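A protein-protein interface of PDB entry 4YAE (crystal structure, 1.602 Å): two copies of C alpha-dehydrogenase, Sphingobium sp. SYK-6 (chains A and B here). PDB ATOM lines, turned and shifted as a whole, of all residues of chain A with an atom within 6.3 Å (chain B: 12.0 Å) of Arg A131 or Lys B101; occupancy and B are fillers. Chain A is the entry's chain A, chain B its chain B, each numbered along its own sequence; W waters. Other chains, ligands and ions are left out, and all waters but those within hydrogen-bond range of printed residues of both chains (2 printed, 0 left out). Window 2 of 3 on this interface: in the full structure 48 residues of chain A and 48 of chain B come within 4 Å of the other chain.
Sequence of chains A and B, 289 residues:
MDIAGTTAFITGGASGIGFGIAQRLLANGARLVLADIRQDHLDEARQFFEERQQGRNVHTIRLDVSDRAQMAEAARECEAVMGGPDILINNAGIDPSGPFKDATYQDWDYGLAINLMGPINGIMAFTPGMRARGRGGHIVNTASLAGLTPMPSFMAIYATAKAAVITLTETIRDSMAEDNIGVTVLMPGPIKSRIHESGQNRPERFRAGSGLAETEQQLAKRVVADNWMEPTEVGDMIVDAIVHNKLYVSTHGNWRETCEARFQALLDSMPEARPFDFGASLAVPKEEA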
ATOM      1  N   MET A 124     -16.181 -16.982   0.658  1.00  0.00           N
ATOM      2  CA  MET A 124     -15.305 -16.798   1.814  1.00  0.00           C
ATOM      3  C   MET A 124     -16.053 -16.277   3.044  1.00  0.00           C
ATOM      4  O   MET A 124     -15.833 -16.744   4.166  1.00  0.00           O
ATOM      5  CB  MET A 124     -14.172 -15.827   1.466  1.00  0.00           C
ATOM      6  CG  MET A 124     -13.146 -16.374   0.482  1.00  0.00           C
ATOM      7  SD  MET A 124     -12.177 -17.776   1.094  1.00  0.00           S
ATOM      8  CE  MET A 124     -11.931 -17.347   2.748  1.00  0.00           C
ATOM      9  N   PHE A 126     -19.504 -16.195   3.638  1.00  0.00           N
ATOM     10  CA  PHE A 126     -20.735 -16.847   4.063  1.00  0.00           C
ATOM     11  C   PHE A 126     -20.575 -18.326   4.436  1.00  0.00           C
ATOM     12  O   PHE A 126     -21.338 -18.828   5.251  1.00  0.00           O
ATOM     13  CB  PHE A 126     -21.814 -16.722   2.976  1.00  0.00           C
ATOM     14  CG  PHE A 126     -22.466 -15.368   2.914  1.00  0.00           C
ATOM     15  CD1 PHE A 126     -21.927 -14.342   2.153  1.00  0.00           C
ATOM     16  CD2 PHE A 126     -23.628 -15.119   3.617  1.00  0.00           C
ATOM     17  CE1 PHE A 126     -22.532 -13.112   2.097  1.00  0.00           C
ATOM     18  CE2 PHE A 126     -24.240 -13.887   3.563  1.00  0.00           C
ATOM     19  CZ  PHE A 126     -23.694 -12.880   2.803  1.00  0.00           C
ATOM     20  N   THR A 127     -19.602 -19.038   3.869  1.00  0.00           N
ATOM     21  CA  THR A 127     -19.569 -20.482   4.111  1.00  0.00           C
ATOM     22  C   THR A 127     -19.148 -20.869   5.545  1.00  0.00           C
ATOM     23  O   THR A 127     -19.565 -21.917   6.023  1.00  0.00           O
ATOM     24  CB  THR A 127     -18.662 -21.234   3.083  1.00  0.00           C
ATOM     25  OG1 THR A 127     -17.343 -20.683   3.062  1.00  0.00           O
ATOM     26  CG2 THR A 127     -19.258 -21.149   1.693  1.00  0.00           C
ATOM     27  N   PRO A 128     -18.352 -20.036   6.255  1.00  0.00           N
ATOM     28  CA  PRO A 128     -18.086 -20.484   7.632  1.00  0.00           C
ATOM     29  C   PRO A 128     -19.377 -20.698   8.430  1.00  0.00           C
ATOM     30  O   PRO A 128     -19.536 -21.730   9.082  1.00  0.00           O
ATOM     31  CB  PRO A 128     -17.233 -19.344   8.212  1.00  0.00           C
ATOM     32  CG  PRO A 128     -16.507 -18.811   7.021  1.00  0.00           C
ATOM     33  CD  PRO A 128     -17.498 -18.896   5.875  1.00  0.00           C
ATOM     34  N   GLY A 129     -20.307 -19.752   8.337  1.00  0.00           N
ATOM     35  CA  GLY A 129     -21.588 -19.889   9.009  1.00  0.00           C
ATOM     36  C   GLY A 129     -22.469 -20.966   8.409  1.00  0.00           C
ATOM     37  O   GLY A 129     -23.140 -21.710   9.127  1.00  0.00           O
ATOM     38  N   MET A 130     -22.486 -21.052   7.087  1.00  0.00           N
ATOM     39  CA  MET A 130     -23.324 -22.054   6.424  1.00  0.00           C
ATOM     40  C   MET A 130     -22.875 -23.458   6.815  1.00  0.00           C
ATOM     41  O   MET A 130     -23.699 -24.336   7.060  1.00  0.00           O
ATOM     42  CB  MET A 130     -23.282 -21.885   4.909  1.00  0.00           C
ATOM     43  CG  MET A 130     -23.905 -20.592   4.412  1.00  0.00           C
ATOM     44  SD  MET A 130     -23.701 -20.351   2.631  1.00  0.00           S
ATOM     45  CE  MET A 130     -24.611 -21.788   2.070  1.00  0.00           C
ATOM     46  N   ARG A 131     -21.568 -23.667   6.893  1.00  0.00           N
ATOM     47  CA  ARG A 131     -21.029 -24.948   7.363  1.00  0.00           C
ATOM     48  C   ARG A 131     -21.351 -25.186   8.841  1.00  0.00           C
ATOM     49  O   ARG A 131     -21.835 -26.250   9.220  1.00  0.00           O
ATOM     50  CB  ARG A 131     -19.511 -25.009   7.157  1.00  0.00           C
ATOM     51  CG  ARG A 131     -19.041 -25.000   5.717  1.00  0.00           C
ATOM     52  CD  ARG A 131     -17.517 -25.193   5.685  1.00  0.00           C
ATOM     53  NE  ARG A 131     -16.883 -24.914   4.400  1.00  0.00           N
ATOM     54  CZ  ARG A 131     -16.748 -25.795   3.412  1.00  0.00           C
ATOM     55  NH1 ARG A 131     -17.256 -27.024   3.514  1.00  0.00           N
ATOM     56  NH2 ARG A 131     -16.111 -25.440   2.307  1.00  0.00           N
ATOM     57  N   ALA A 132     -21.060 -24.193   9.679  1.00  0.00           N
ATOM     58  CA  ALA A 132     -21.198 -24.348  11.127  1.00  0.00           C
ATOM     59  C   ALA A 132     -22.633 -24.585  11.587  1.00  0.00           C
ATOM     60  O   ALA A 132     -22.860 -25.331  12.536  1.00  0.00           O
ATOM     61  CB  ALA A 132     -20.634 -23.131  11.834  1.00  0.00           C
ATOM     62  N   ARG A 133     -23.598 -23.924  10.949  1.00  0.00           N
ATOM     63  CA  ARG A 133     -24.987 -24.042  11.376  1.00  0.00           C
ATOM     64  C   ARG A 133     -25.510 -25.448  11.130  1.00  0.00           C
ATOM     65  O   ARG A 133     -26.456 -25.888  11.780  1.00  0.00           O
ATOM     66  CB  ARG A 133     -25.863 -23.000  10.673  1.00  0.00           C
ATOM     67  CG  ARG A 133     -25.638 -21.592  11.220  1.00  0.00           C
ATOM     68  CD  ARG A 133     -26.624 -20.574  10.660  1.00  0.00           C
ATOM     69  NE  ARG A 133     -26.466 -20.364   9.223  1.00  0.00           N
ATOM     70  CZ  ARG A 133     -25.611 -19.510   8.669  1.00  0.00           C
ATOM     71  NH1 ARG A 133     -24.795 -18.777   9.422  1.00  0.00           N
ATOM     72  NH2 ARG A 133     -25.568 -19.399   7.348  1.00  0.00           N
ATOM     73  N   GLY A 134     -24.894 -26.155  10.187  1.00  0.00           N
ATOM     74  CA  GLY A 134     -25.132 -27.573  10.032  1.00  0.00           C
ATOM     75  C   GLY A 134     -26.478 -27.976   9.471  1.00  0.00           C
ATOM     76  O   GLY A 134     -26.877 -29.124   9.641  1.00  0.00           O
ATOM     77  N   ARG A 135     -27.174 -27.071   8.790  1.00  0.00           N
ATOM     78  CA  ARG A 135     -28.446 -27.453   8.175  1.00  0.00           C
ATOM     79  C   ARG A 135     -28.367 -27.444   6.650  1.00  0.00           C
ATOM     80  O   ARG A 135     -29.386 -27.411   5.957  1.00  0.00           O
ATOM     81  CB  ARG A 135     -29.587 -26.559   8.672  1.00  0.00           C
ATOM     82  CG  ARG A 135     -29.423 -25.081   8.498  1.00  0.00           C
ATOM     83  CD  ARG A 135     -30.575 -24.364   9.213  1.00  0.00           C
ATOM     84  NE  ARG A 135     -30.559 -22.916   9.025  1.00  0.00           N
ATOM     85  CZ  ARG A 135     -30.190 -22.026   9.947  1.00  0.00           C
ATOM     86  NH1 ARG A 135     -29.798 -22.408  11.161  1.00  0.00           N
ATOM     87  NH2 ARG A 135     -30.221 -20.734   9.652  1.00  0.00           N
ATOM     88  N   GLY A 136     -27.146 -27.539   6.137  1.00  0.00           N
ATOM     89  CA  GLY A 136     -26.927 -27.588   4.706  1.00  0.00           C
ATOM     90  C   GLY A 136     -27.129 -26.227   4.093  1.00  0.00           C
ATOM     91  O   GLY A 136     -27.245 -25.218   4.783  1.00  0.00           O
ATOM     92  N   ILE A 172     -15.328 -26.541  -6.327  1.00  0.00           N
ATOM     93  CA  ILE A 172     -15.615 -26.495  -4.893  1.00  0.00           C
ATOM     94  C   ILE A 172     -16.740 -27.444  -4.480  1.00  0.00           C
ATOM     95  O   ILE A 172     -17.038 -27.570  -3.292  1.00  0.00           O
ATOM     96  CB  ILE A 172     -16.002 -25.081  -4.418  1.00  0.00           C
ATOM     97  CG1 ILE A 172     -17.308 -24.620  -5.080  1.00  0.00           C
ATOM     98  CG2 ILE A 172     -14.852 -24.097  -4.659  1.00  0.00           C
ATOM     99  CD1 ILE A 172     -17.808 -23.265  -4.587  1.00  0.00           C
ATOM    100  N   SER A 175     -15.990 -30.043  -1.639  1.00  0.00           N
ATOM    101  CA  SER A 175     -15.720 -29.400  -0.355  1.00  0.00           C
ATOM    102  C   SER A 175     -17.027 -28.957   0.301  1.00  0.00           C
ATOM    103  O   SER A 175     -17.240 -29.159   1.492  1.00  0.00           O
ATOM    104  CB  SER A 175     -14.790 -28.203  -0.535  1.00  0.00           C
ATOM    105  OG  SER A 175     -14.708 -27.458   0.667  1.00  0.00           O
ATOM    106  N   MET A 176     -17.902 -28.358  -0.495  1.00  0.00           N
ATOM    107  CA  MET A 176     -19.186 -27.882   0.007  1.00  0.00           C
ATOM    108  C   MET A 176     -20.090 -29.046   0.400  1.00  0.00           C
ATOM    109  O   MET A 176     -20.817 -28.972   1.392  1.00  0.00           O
ATOM    110  CB  MET A 176     -19.863 -26.994  -1.046  1.00  0.00           C
ATOM    111  CG  MET A 176     -19.066 -25.749  -1.397  1.00  0.00           C
ATOM    112  SD  MET A 176     -18.789 -24.717   0.051  1.00  0.00           S
ATOM    113  CE  MET A 176     -17.442 -23.712  -0.556  1.00  0.00           C
ATOM    114  N   ALA A 177     -20.023 -30.137  -0.361  1.00  0.00           N
ATOM    115  CA  ALA A 177     -20.866 -31.306  -0.102  1.00  0.00           C
ATOM    116  C   ALA A 177     -20.582 -31.912   1.268  1.00  0.00           C
ATOM    117  O   ALA A 177     -21.454 -32.544   1.868  1.00  0.00           O
ATOM    118  CB  ALA A 177     -20.659 -32.349  -1.188  1.00  0.00           C
ATOM    119  N   GLU A 178     -19.356 -31.736   1.763  1.00  0.00           N
ATOM    120  CA  GLU A 178     -18.990 -32.268   3.067  1.00  0.00           C
ATOM    121  C   GLU A 178     -19.922 -31.753   4.153  1.00  0.00           C
ATOM    122  O   GLU A 178     -20.161 -32.439   5.143  1.00  0.00           O
ATOM    123  CB  GLU A 178     -17.552 -31.904   3.419  1.00  0.00           C
ATOM    124  CG  GLU A 178     -16.502 -32.555   2.542  1.00  0.00           C
ATOM    125  CD  GLU A 178     -15.093 -32.241   3.000  1.00  0.00           C
ATOM    126  OE1 GLU A 178     -14.943 -31.634   4.084  1.00  0.00           O
ATOM    127  OE2 GLU A 178     -14.140 -32.591   2.274  1.00  0.00           O
ATOM    128  N   ASP A 179     -20.433 -30.539   3.956  1.00  0.00           N
ATOM    129  CA  ASP A 179     -21.349 -29.914   4.901  1.00  0.00           C
ATOM    130  C   ASP A 179     -22.745 -29.767   4.312  1.00  0.00           C
ATOM    131  O   ASP A 179     -23.510 -28.897   4.711  1.00  0.00           O
ATOM    132  CB  ASP A 179     -20.790 -28.560   5.331  1.00  0.00           C
ATOM    133  CG  ASP A 179     -19.543 -28.710   6.175  1.00  0.00           C
ATOM    134  OD1 ASP A 179     -19.667 -29.209   7.312  1.00  0.00           O
ATOM    135  OD2 ASP A 179     -18.448 -28.359   5.703  1.00  0.00           O
ATOM    136  N   ILE A 181     -23.807 -28.715   1.524  1.00  0.00           N
ATOM    137  CA  ILE A 181     -24.029 -27.491   0.752  1.00  0.00           C
ATOM    138  C   ILE A 181     -23.864 -27.823  -0.727  1.00  0.00           C
ATOM    139  O   ILE A 181     -22.782 -28.216  -1.153  1.00  0.00           O
ATOM    140  CB  ILE A 181     -23.052 -26.371   1.147  1.00  0.00           C
ATOM    141  CG1 ILE A 181     -23.247 -25.971   2.610  1.00  0.00           C
ATOM    142  CG2 ILE A 181     -23.236 -25.141   0.257  1.00  0.00           C
ATOM    143  CD1 ILE A 181     -22.093 -25.177   3.185  1.00  0.00           C
ATOM    144  N   PRO B  96      -1.224 -22.791  -4.963  1.00  0.00           N
ATOM    145  CA  PRO B  96      -1.568 -22.564  -3.559  1.00  0.00           C
ATOM    146  C   PRO B  96      -2.562 -23.597  -3.027  1.00  0.00           C
ATOM    147  O   PRO B  96      -3.366 -23.286  -2.147  1.00  0.00           O
ATOM    148  CB  PRO B  96      -2.192 -21.167  -3.592  1.00  0.00           C
ATOM    149  CG  PRO B  96      -2.869 -21.127  -4.905  1.00  0.00           C
ATOM    150  CD  PRO B  96      -2.064 -21.976  -5.857  1.00  0.00           C
ATOM    151  N   SER B  97      -2.493 -24.819  -3.546  1.00  0.00           N
ATOM    152  CA  SER B  97      -3.471 -25.846  -3.201  1.00  0.00           C
ATOM    153  C   SER B  97      -3.410 -26.249  -1.734  1.00  0.00           C
ATOM    154  O   SER B  97      -2.381 -26.119  -1.072  1.00  0.00           O
ATOM    155  CB  SER B  97      -3.276 -27.083  -4.080  1.00  0.00           C
ATOM    156  OG  SER B  97      -3.648 -26.807  -5.423  1.00  0.00           O
ATOM    157  N   GLY B  98      -4.539 -26.746  -1.249  1.00  0.00           N
ATOM    158  CA  GLY B  98      -4.696 -27.196   0.119  1.00  0.00           C
ATOM    159  C   GLY B  98      -6.181 -27.358   0.360  1.00  0.00           C
ATOM    160  O   GLY B  98      -6.975 -26.957  -0.493  1.00  0.00           O
ATOM    161  N   PRO B  99      -6.574 -27.947   1.502  1.00  0.00           N
ATOM    162  CA  PRO B  99      -7.990 -28.153   1.829  1.00  0.00           C
ATOM    163  C   PRO B  99      -8.793 -26.878   1.600  1.00  0.00           C
ATOM    164  O   PRO B  99      -8.399 -25.824   2.119  1.00  0.00           O
ATOM    165  CB  PRO B  99      -7.957 -28.536   3.311  1.00  0.00           C
ATOM    166  CG  PRO B  99      -6.626 -29.165   3.493  1.00  0.00           C
ATOM    167  CD  PRO B  99      -5.685 -28.431   2.571  1.00  0.00           C
ATOM    168  N   PHE B 100      -9.874 -26.946   0.829  1.00  0.00           N
ATOM    169  CA  PHE B 100     -10.488 -25.712   0.380  1.00  0.00           C
ATOM    170  C   PHE B 100     -11.083 -24.949   1.554  1.00  0.00           C
ATOM    171  O   PHE B 100     -11.070 -23.719   1.558  1.00  0.00           O
ATOM    172  CB  PHE B 100     -11.560 -25.947  -0.679  1.00  0.00           C
ATOM    173  CG  PHE B 100     -12.124 -24.671  -1.217  1.00  0.00           C
ATOM    174  CD1 PHE B 100     -11.339 -23.841  -2.003  1.00  0.00           C
ATOM    175  CD2 PHE B 100     -13.411 -24.256  -0.885  1.00  0.00           C
ATOM    176  CE1 PHE B 100     -11.827 -22.641  -2.472  1.00  0.00           C
ATOM    177  CE2 PHE B 100     -13.909 -23.049  -1.361  1.00  0.00           C
ATOM    178  CZ  PHE B 100     -13.117 -22.243  -2.145  1.00  0.00           C
ATOM    179  N   LYS B 101     -11.574 -25.676   2.553  1.00  0.00           N
ATOM    180  CA  LYS B 101     -12.086 -25.048   3.768  1.00  0.00           C
ATOM    181  C   LYS B 101     -11.090 -24.087   4.397  1.00  0.00           C
ATOM    182  O   LYS B 101     -11.489 -23.084   4.992  1.00  0.00           O
ATOM    183  CB  LYS B 101     -12.464 -26.103   4.808  1.00  0.00           C
ATOM    184  CG  LYS B 101     -13.835 -26.655   4.636  1.00  0.00           C
ATOM    185  CD  LYS B 101     -14.347 -27.259   5.931  1.00  0.00           C
ATOM    186  CE  LYS B 101     -13.403 -28.313   6.488  1.00  0.00           C
ATOM    187  NZ  LYS B 101     -13.974 -28.945   7.709  1.00  0.00           N
ATOM    188  N   ASP B 102      -9.802 -24.401   4.271  1.00  0.00           N
ATOM    189  CA  ASP B 102      -8.747 -23.629   4.906  1.00  0.00           C
ATOM    190  C   ASP B 102      -8.158 -22.553   4.001  1.00  0.00           C
ATOM    191  O   ASP B 102      -7.193 -21.899   4.379  1.00  0.00           O
ATOM    192  CB  ASP B 102      -7.611 -24.546   5.361  1.00  0.00           C
ATOM    193  CG  ASP B 102      -8.029 -25.506   6.456  1.00  0.00           C
ATOM    194  OD1 ASP B 102      -8.899 -25.149   7.280  1.00  0.00           O
ATOM    195  OD2 ASP B 102      -7.470 -26.621   6.498  1.00  0.00           O
ATOM    196  N   ALA B 103      -8.722 -22.385   2.809  1.00  0.00           N
ATOM    197  CA  ALA B 103      -8.244 -21.365   1.882  1.00  0.00           C
ATOM    198  C   ALA B 103      -8.392 -19.983   2.511  1.00  0.00           C
ATOM    199  O   ALA B 103      -9.363 -19.713   3.218  1.00  0.00           O
ATOM    200  CB  ALA B 103      -9.006 -21.438   0.568  1.00  0.00           C
ATOM    201  N   THR B 104      -7.399 -19.135   2.276  1.00  0.00           N
ATOM    202  CA  THR B 104      -7.424 -17.761   2.759  1.00  0.00           C
ATOM    203  C   THR B 104      -7.541 -16.795   1.595  1.00  0.00           C
ATOM    204  O   THR B 104      -7.303 -17.162   0.448  1.00  0.00           O
ATOM    205  CB  THR B 104      -6.157 -17.418   3.537  1.00  0.00           C
ATOM    206  OG1 THR B 104      -5.040 -17.495   2.646  1.00  0.00           O
ATOM    207  CG2 THR B 104      -5.967 -18.382   4.698  1.00  0.00           C
ATOM    208  N   TYR B 105      -7.905 -15.553   1.905  1.00  0.00           N
ATOM    209  CA  TYR B 105      -7.891 -14.496   0.910  1.00  0.00           C
ATOM    210  C   TYR B 105      -6.492 -14.341   0.317  1.00  0.00           C
ATOM    211  O   TYR B 105      -6.357 -14.107  -0.881  1.00  0.00           O
ATOM    212  CB  TYR B 105      -8.369 -13.178   1.516  1.00  0.00           C
ATOM    213  CG  TYR B 105      -9.878 -12.991   1.511  1.00  0.00           C
ATOM    214  CD1 TYR B 105     -10.628 -13.216   0.360  1.00  0.00           C
ATOM    215  CD2 TYR B 105     -10.540 -12.574   2.650  1.00  0.00           C
ATOM    216  CE1 TYR B 105     -11.995 -13.030   0.352  1.00  0.00           C
ATOM    217  CE2 TYR B 105     -11.913 -12.389   2.654  1.00  0.00           C
ATOM    218  CZ  TYR B 105     -12.633 -12.609   1.505  1.00  0.00           C
ATOM    219  OH  TYR B 105     -13.997 -12.410   1.530  1.00  0.00           O
ATOM    220  N   GLN B 106      -5.459 -14.490   1.145  1.00  0.00           N
ATOM    221  CA  GLN B 106      -4.085 -14.452   0.632  1.00  0.00           C
ATOM    222  C   GLN B 106      -3.805 -15.554  -0.401  1.00  0.00           C
ATOM    223  O   GLN B 106      -3.146 -15.305  -1.413  1.00  0.00           O
ATOM    224  CB  GLN B 106      -3.084 -14.554   1.786  1.00  0.00           C
ATOM    225  CG  GLN B 106      -2.935 -13.278   2.600  1.00  0.00           C
ATOM    226  CD  GLN B 106      -1.999 -12.276   1.944  1.00  0.00           C
ATOM    227  OE1 GLN B 106      -2.014 -12.098   0.724  1.00  0.00           O
ATOM    228  NE2 GLN B 106      -1.169 -11.622   2.752  1.00  0.00           N
ATOM    229  N   ASP B 107      -4.309 -16.767  -0.159  1.00  0.00           N
ATOM    230  CA  ASP B 107      -4.151 -17.867  -1.114  1.00  0.00           C
ATOM    231  C   ASP B 107      -4.778 -17.499  -2.446  1.00  0.00           C
ATOM    232  O   ASP B 107      -4.203 -17.715  -3.516  1.00  0.00           O
ATOM    233  CB  ASP B 107      -4.812 -19.158  -0.619  1.00  0.00           C
ATOM    234  CG  ASP B 107      -4.145 -19.755   0.601  1.00  0.00           C
ATOM    235  OD1 ASP B 107      -2.946 -19.502   0.846  1.00  0.00           O
ATOM    236  OD2 ASP B 107      -4.847 -20.507   1.316  1.00  0.00           O
ATOM    237  N   TRP B 108      -5.997 -16.971  -2.386  1.00  0.00           N
ATOM    238  CA  TRP B 108      -6.687 -16.580  -3.597  1.00  0.00           C
ATOM    239  C   TRP B 108      -5.959 -15.455  -4.316  1.00  0.00           C
ATOM    240  O   TRP B 108      -5.800 -15.482  -5.529  1.00  0.00           O
ATOM    241  CB  TRP B 108      -8.118 -16.130  -3.288  1.00  0.00           C
ATOM    242  CG  TRP B 108      -9.113 -17.213  -3.345  1.00  0.00           C
ATOM    243  CD1 TRP B 108      -9.805 -17.735  -2.304  1.00  0.00           C
ATOM    244  CD2 TRP B 108      -9.534 -17.922  -4.513  1.00  0.00           C
ATOM    245  NE1 TRP B 108     -10.643 -18.731  -2.747  1.00  0.00           N
ATOM    246  CE2 TRP B 108     -10.494 -18.864  -4.102  1.00  0.00           C
ATOM    247  CE3 TRP B 108      -9.195 -17.849  -5.862  1.00  0.00           C
ATOM    248  CZ2 TRP B 108     -11.118 -19.734  -4.996  1.00  0.00           C
ATOM    249  CZ3 TRP B 108      -9.814 -18.716  -6.753  1.00  0.00           C
ATOM    250  CH2 TRP B 108     -10.770 -19.639  -6.314  1.00  0.00           C
ATOM    251  N   PRO B 152     -10.291 -31.921  -8.055  1.00  0.00           N
ATOM    252  CA  PRO B 152     -10.763 -31.941  -6.669  1.00  0.00           C
ATOM    253  C   PRO B 152     -10.716 -30.551  -6.038  1.00  0.00           C
ATOM    254  O   PRO B 152      -9.994 -29.678  -6.523  1.00  0.00           O
ATOM    255  CB  PRO B 152      -9.789 -32.892  -5.985  1.00  0.00           C
ATOM    256  CG  PRO B 152      -8.550 -32.807  -6.780  1.00  0.00           C
ATOM    257  CD  PRO B 152      -8.975 -32.568  -8.195  1.00  0.00           C
ATOM    258  N   SER B 153     -11.470 -30.355  -4.962  1.00  0.00           N
ATOM    259  CA  SER B 153     -11.632 -29.031  -4.379  1.00  0.00           C
ATOM    260  C   SER B 153     -10.337 -28.444  -3.839  1.00  0.00           C
ATOM    261  O   SER B 153     -10.174 -27.236  -3.793  1.00  0.00           O
ATOM    262  CB  SER B 153     -12.663 -29.076  -3.251  1.00  0.00           C
ATOM    263  OG  SER B 153     -13.921 -29.516  -3.742  1.00  0.00           O
ATOM    264  N   PHE B 154      -9.404 -29.290  -3.425  1.00  0.00           N
ATOM    265  CA  PHE B 154      -8.174 -28.750  -2.866  1.00  0.00           C
ATOM    266  C   PHE B 154      -7.343 -28.051  -3.946  1.00  0.00           C
ATOM    267  O   PHE B 154      -6.403 -27.322  -3.627  1.00  0.00           O
ATOM    268  CB  PHE B 154      -7.378 -29.847  -2.131  1.00  0.00           C
ATOM    269  CG  PHE B 154      -6.621 -30.779  -3.023  1.00  0.00           C
ATOM    270  CD1 PHE B 154      -7.179 -31.975  -3.436  1.00  0.00           C
ATOM    271  CD2 PHE B 154      -5.325 -30.483  -3.408  1.00  0.00           C
ATOM    272  CE1 PHE B 154      -6.463 -32.845  -4.249  1.00  0.00           C
ATOM    273  CE2 PHE B 154      -4.614 -31.345  -4.215  1.00  0.00           C
ATOM    274  CZ  PHE B 154      -5.185 -32.524  -4.633  1.00  0.00           C
ATOM    275  N   MET B 155      -7.713 -28.232  -5.217  1.00  0.00           N
ATOM    276  CA  MET B 155      -7.053 -27.554  -6.328  1.00  0.00           C
ATOM    277  C   MET B 155      -7.893 -26.417  -6.916  1.00  0.00           C
ATOM    278  O   MET B 155      -7.611 -25.955  -8.013  1.00  0.00           O
ATOM    279  CB  MET B 155      -6.735 -28.561  -7.436  1.00  0.00           C
ATOM    280  CG  MET B 155      -5.919 -29.741  -6.955  1.00  0.00           C
ATOM    281  SD  MET B 155      -4.173 -29.413  -7.104  1.00  0.00           S
ATOM    282  CE  MET B 155      -3.951 -29.777  -8.833  1.00  0.00           C
ATOM    283  N   ALA B 156      -8.901 -25.953  -6.178  1.00  0.00           N
ATOM    284  CA  ALA B 156      -9.835 -24.943  -6.699  1.00  0.00           C
ATOM    285  C   ALA B 156      -9.166 -23.666  -7.200  1.00  0.00           C
ATOM    286  O   ALA B 156      -9.545 -23.133  -8.241  1.00  0.00           O
ATOM    287  CB  ALA B 156     -10.870 -24.590  -5.627  1.00  0.00           C
ATOM    288  N   ILE B 157      -8.184 -23.158  -6.472  1.00  0.00           N
ATOM    289  CA  ILE B 157      -7.601 -21.865  -6.825  1.00  0.00           C
ATOM    290  C   ILE B 157      -6.824 -21.984  -8.132  1.00  0.00           C
ATOM    291  O   ILE B 157      -7.012 -21.189  -9.057  1.00  0.00           O
ATOM    292  CB  ILE B 157      -6.700 -21.339  -5.700  1.00  0.00           C
ATOM    293  CG1 ILE B 157      -7.551 -21.109  -4.442  1.00  0.00           C
ATOM    294  CG2 ILE B 157      -6.017 -20.044  -6.118  1.00  0.00           C
ATOM    295  CD1 ILE B 157      -6.766 -20.656  -3.216  1.00  0.00           C
HETATM  296  O   HOH W   1     -16.168 -29.752   6.330  1.00  0.00           O
HETATM  297  O   HOH W   2     -12.720 -28.654   2.064  1.00  0.00           O
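N of Ser A175 lies within hydrogen-bond range of OG of Ser B153, 3.0 Å away.
O of Ser A175 lies within hydrogen-bond range of NH1 of Arg A131. NH1 of Arg A131 lies within salt-bridge range of OD2 of Asp A179 (2.8 Å). The guanidinium group (NH2) of Arg A131 sits at hydrogen-bond distance from the side-chain sulfur (SD) of Met A176, 3.6 Å away. O of Met A176 is in hydrogen-bond range of N of Ile A181 (3.0 Å).
Met A124 touches Ala B103. CB of Met A124 touches OH of Tyr B105, 3.4 Å away. Arg A131 touches Lys B101 (CZ to CG, 3.3 Å). Phe B100 touches Ile A172. Ser B153 touches Ile A172. CB of Phe B100 touches OG of Ser A175, 3.7 Å away. CE of Met A176 touches CE2 of Phe B100, 3.7 Å away.
Printed residues of chain B within 4 Å of Arg A131: Lys B101. Lys B101 touches one residue of chain A. Thr A127 touches none of the printed residues of chain B. No residue of chain B comes within 4 Å of Met A130. No residue of chain B comes within 4 Å of Ala A132. No residue of chain B comes within 4 Å of Gly A134. No residue of chain B comes within 4 Å of Gly A136. Met A176 touches one residue of chain B. No residue of chain B comes within 4 Å of Ala A177. No residue of chain B comes within 4 Å of Glu A178. No residue of chain B comes within 4 Å of Asp A179. Ile A181 touches none of the printed residues of chain B. Of the printed residues of chain A, Ala B103 touches Met A124. Of the printed residues of chain A, Ser B153 touches Ile A172 (3.6 Å) and Ser A175 (3.0 Å). Of the printed residues of chain A, Phe B100 touches Ile A172 (3.6 Å), Ser A175 (3.7 Å) and Met A176 (3.7 Å). The nearest residue of chain A that does not touch Lys B101 is Ser A175 (4.1 Å).
Printed residues of chain A that touch a printed residue of chain B: Met A124, Arg A131, Ile A172, Ser A175 and Met A176. Hydrophobic or aromatic side chains of chain A within 4 Å of the printed part of chain B: Met A124, Ile A172 and Met A176. Among the printed residues, 8 pairs touch across the chains.
No position is printed for both chains. Of the 8 pairs that touch across the chains among the printed residues, none has its exchanged pair printed and touching as well.
Water W2 lies within hydrogen-bond range of the side-chain hydroxyl of Ser A175 and the backbone NH of Lys B101. Water W1 lies within hydrogen-bond range of NZ of Lys B101 (2.7 Å), OD2 of Asp A179 (2.7 Å) and OE1 of Glu A178 (3.2 Å).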
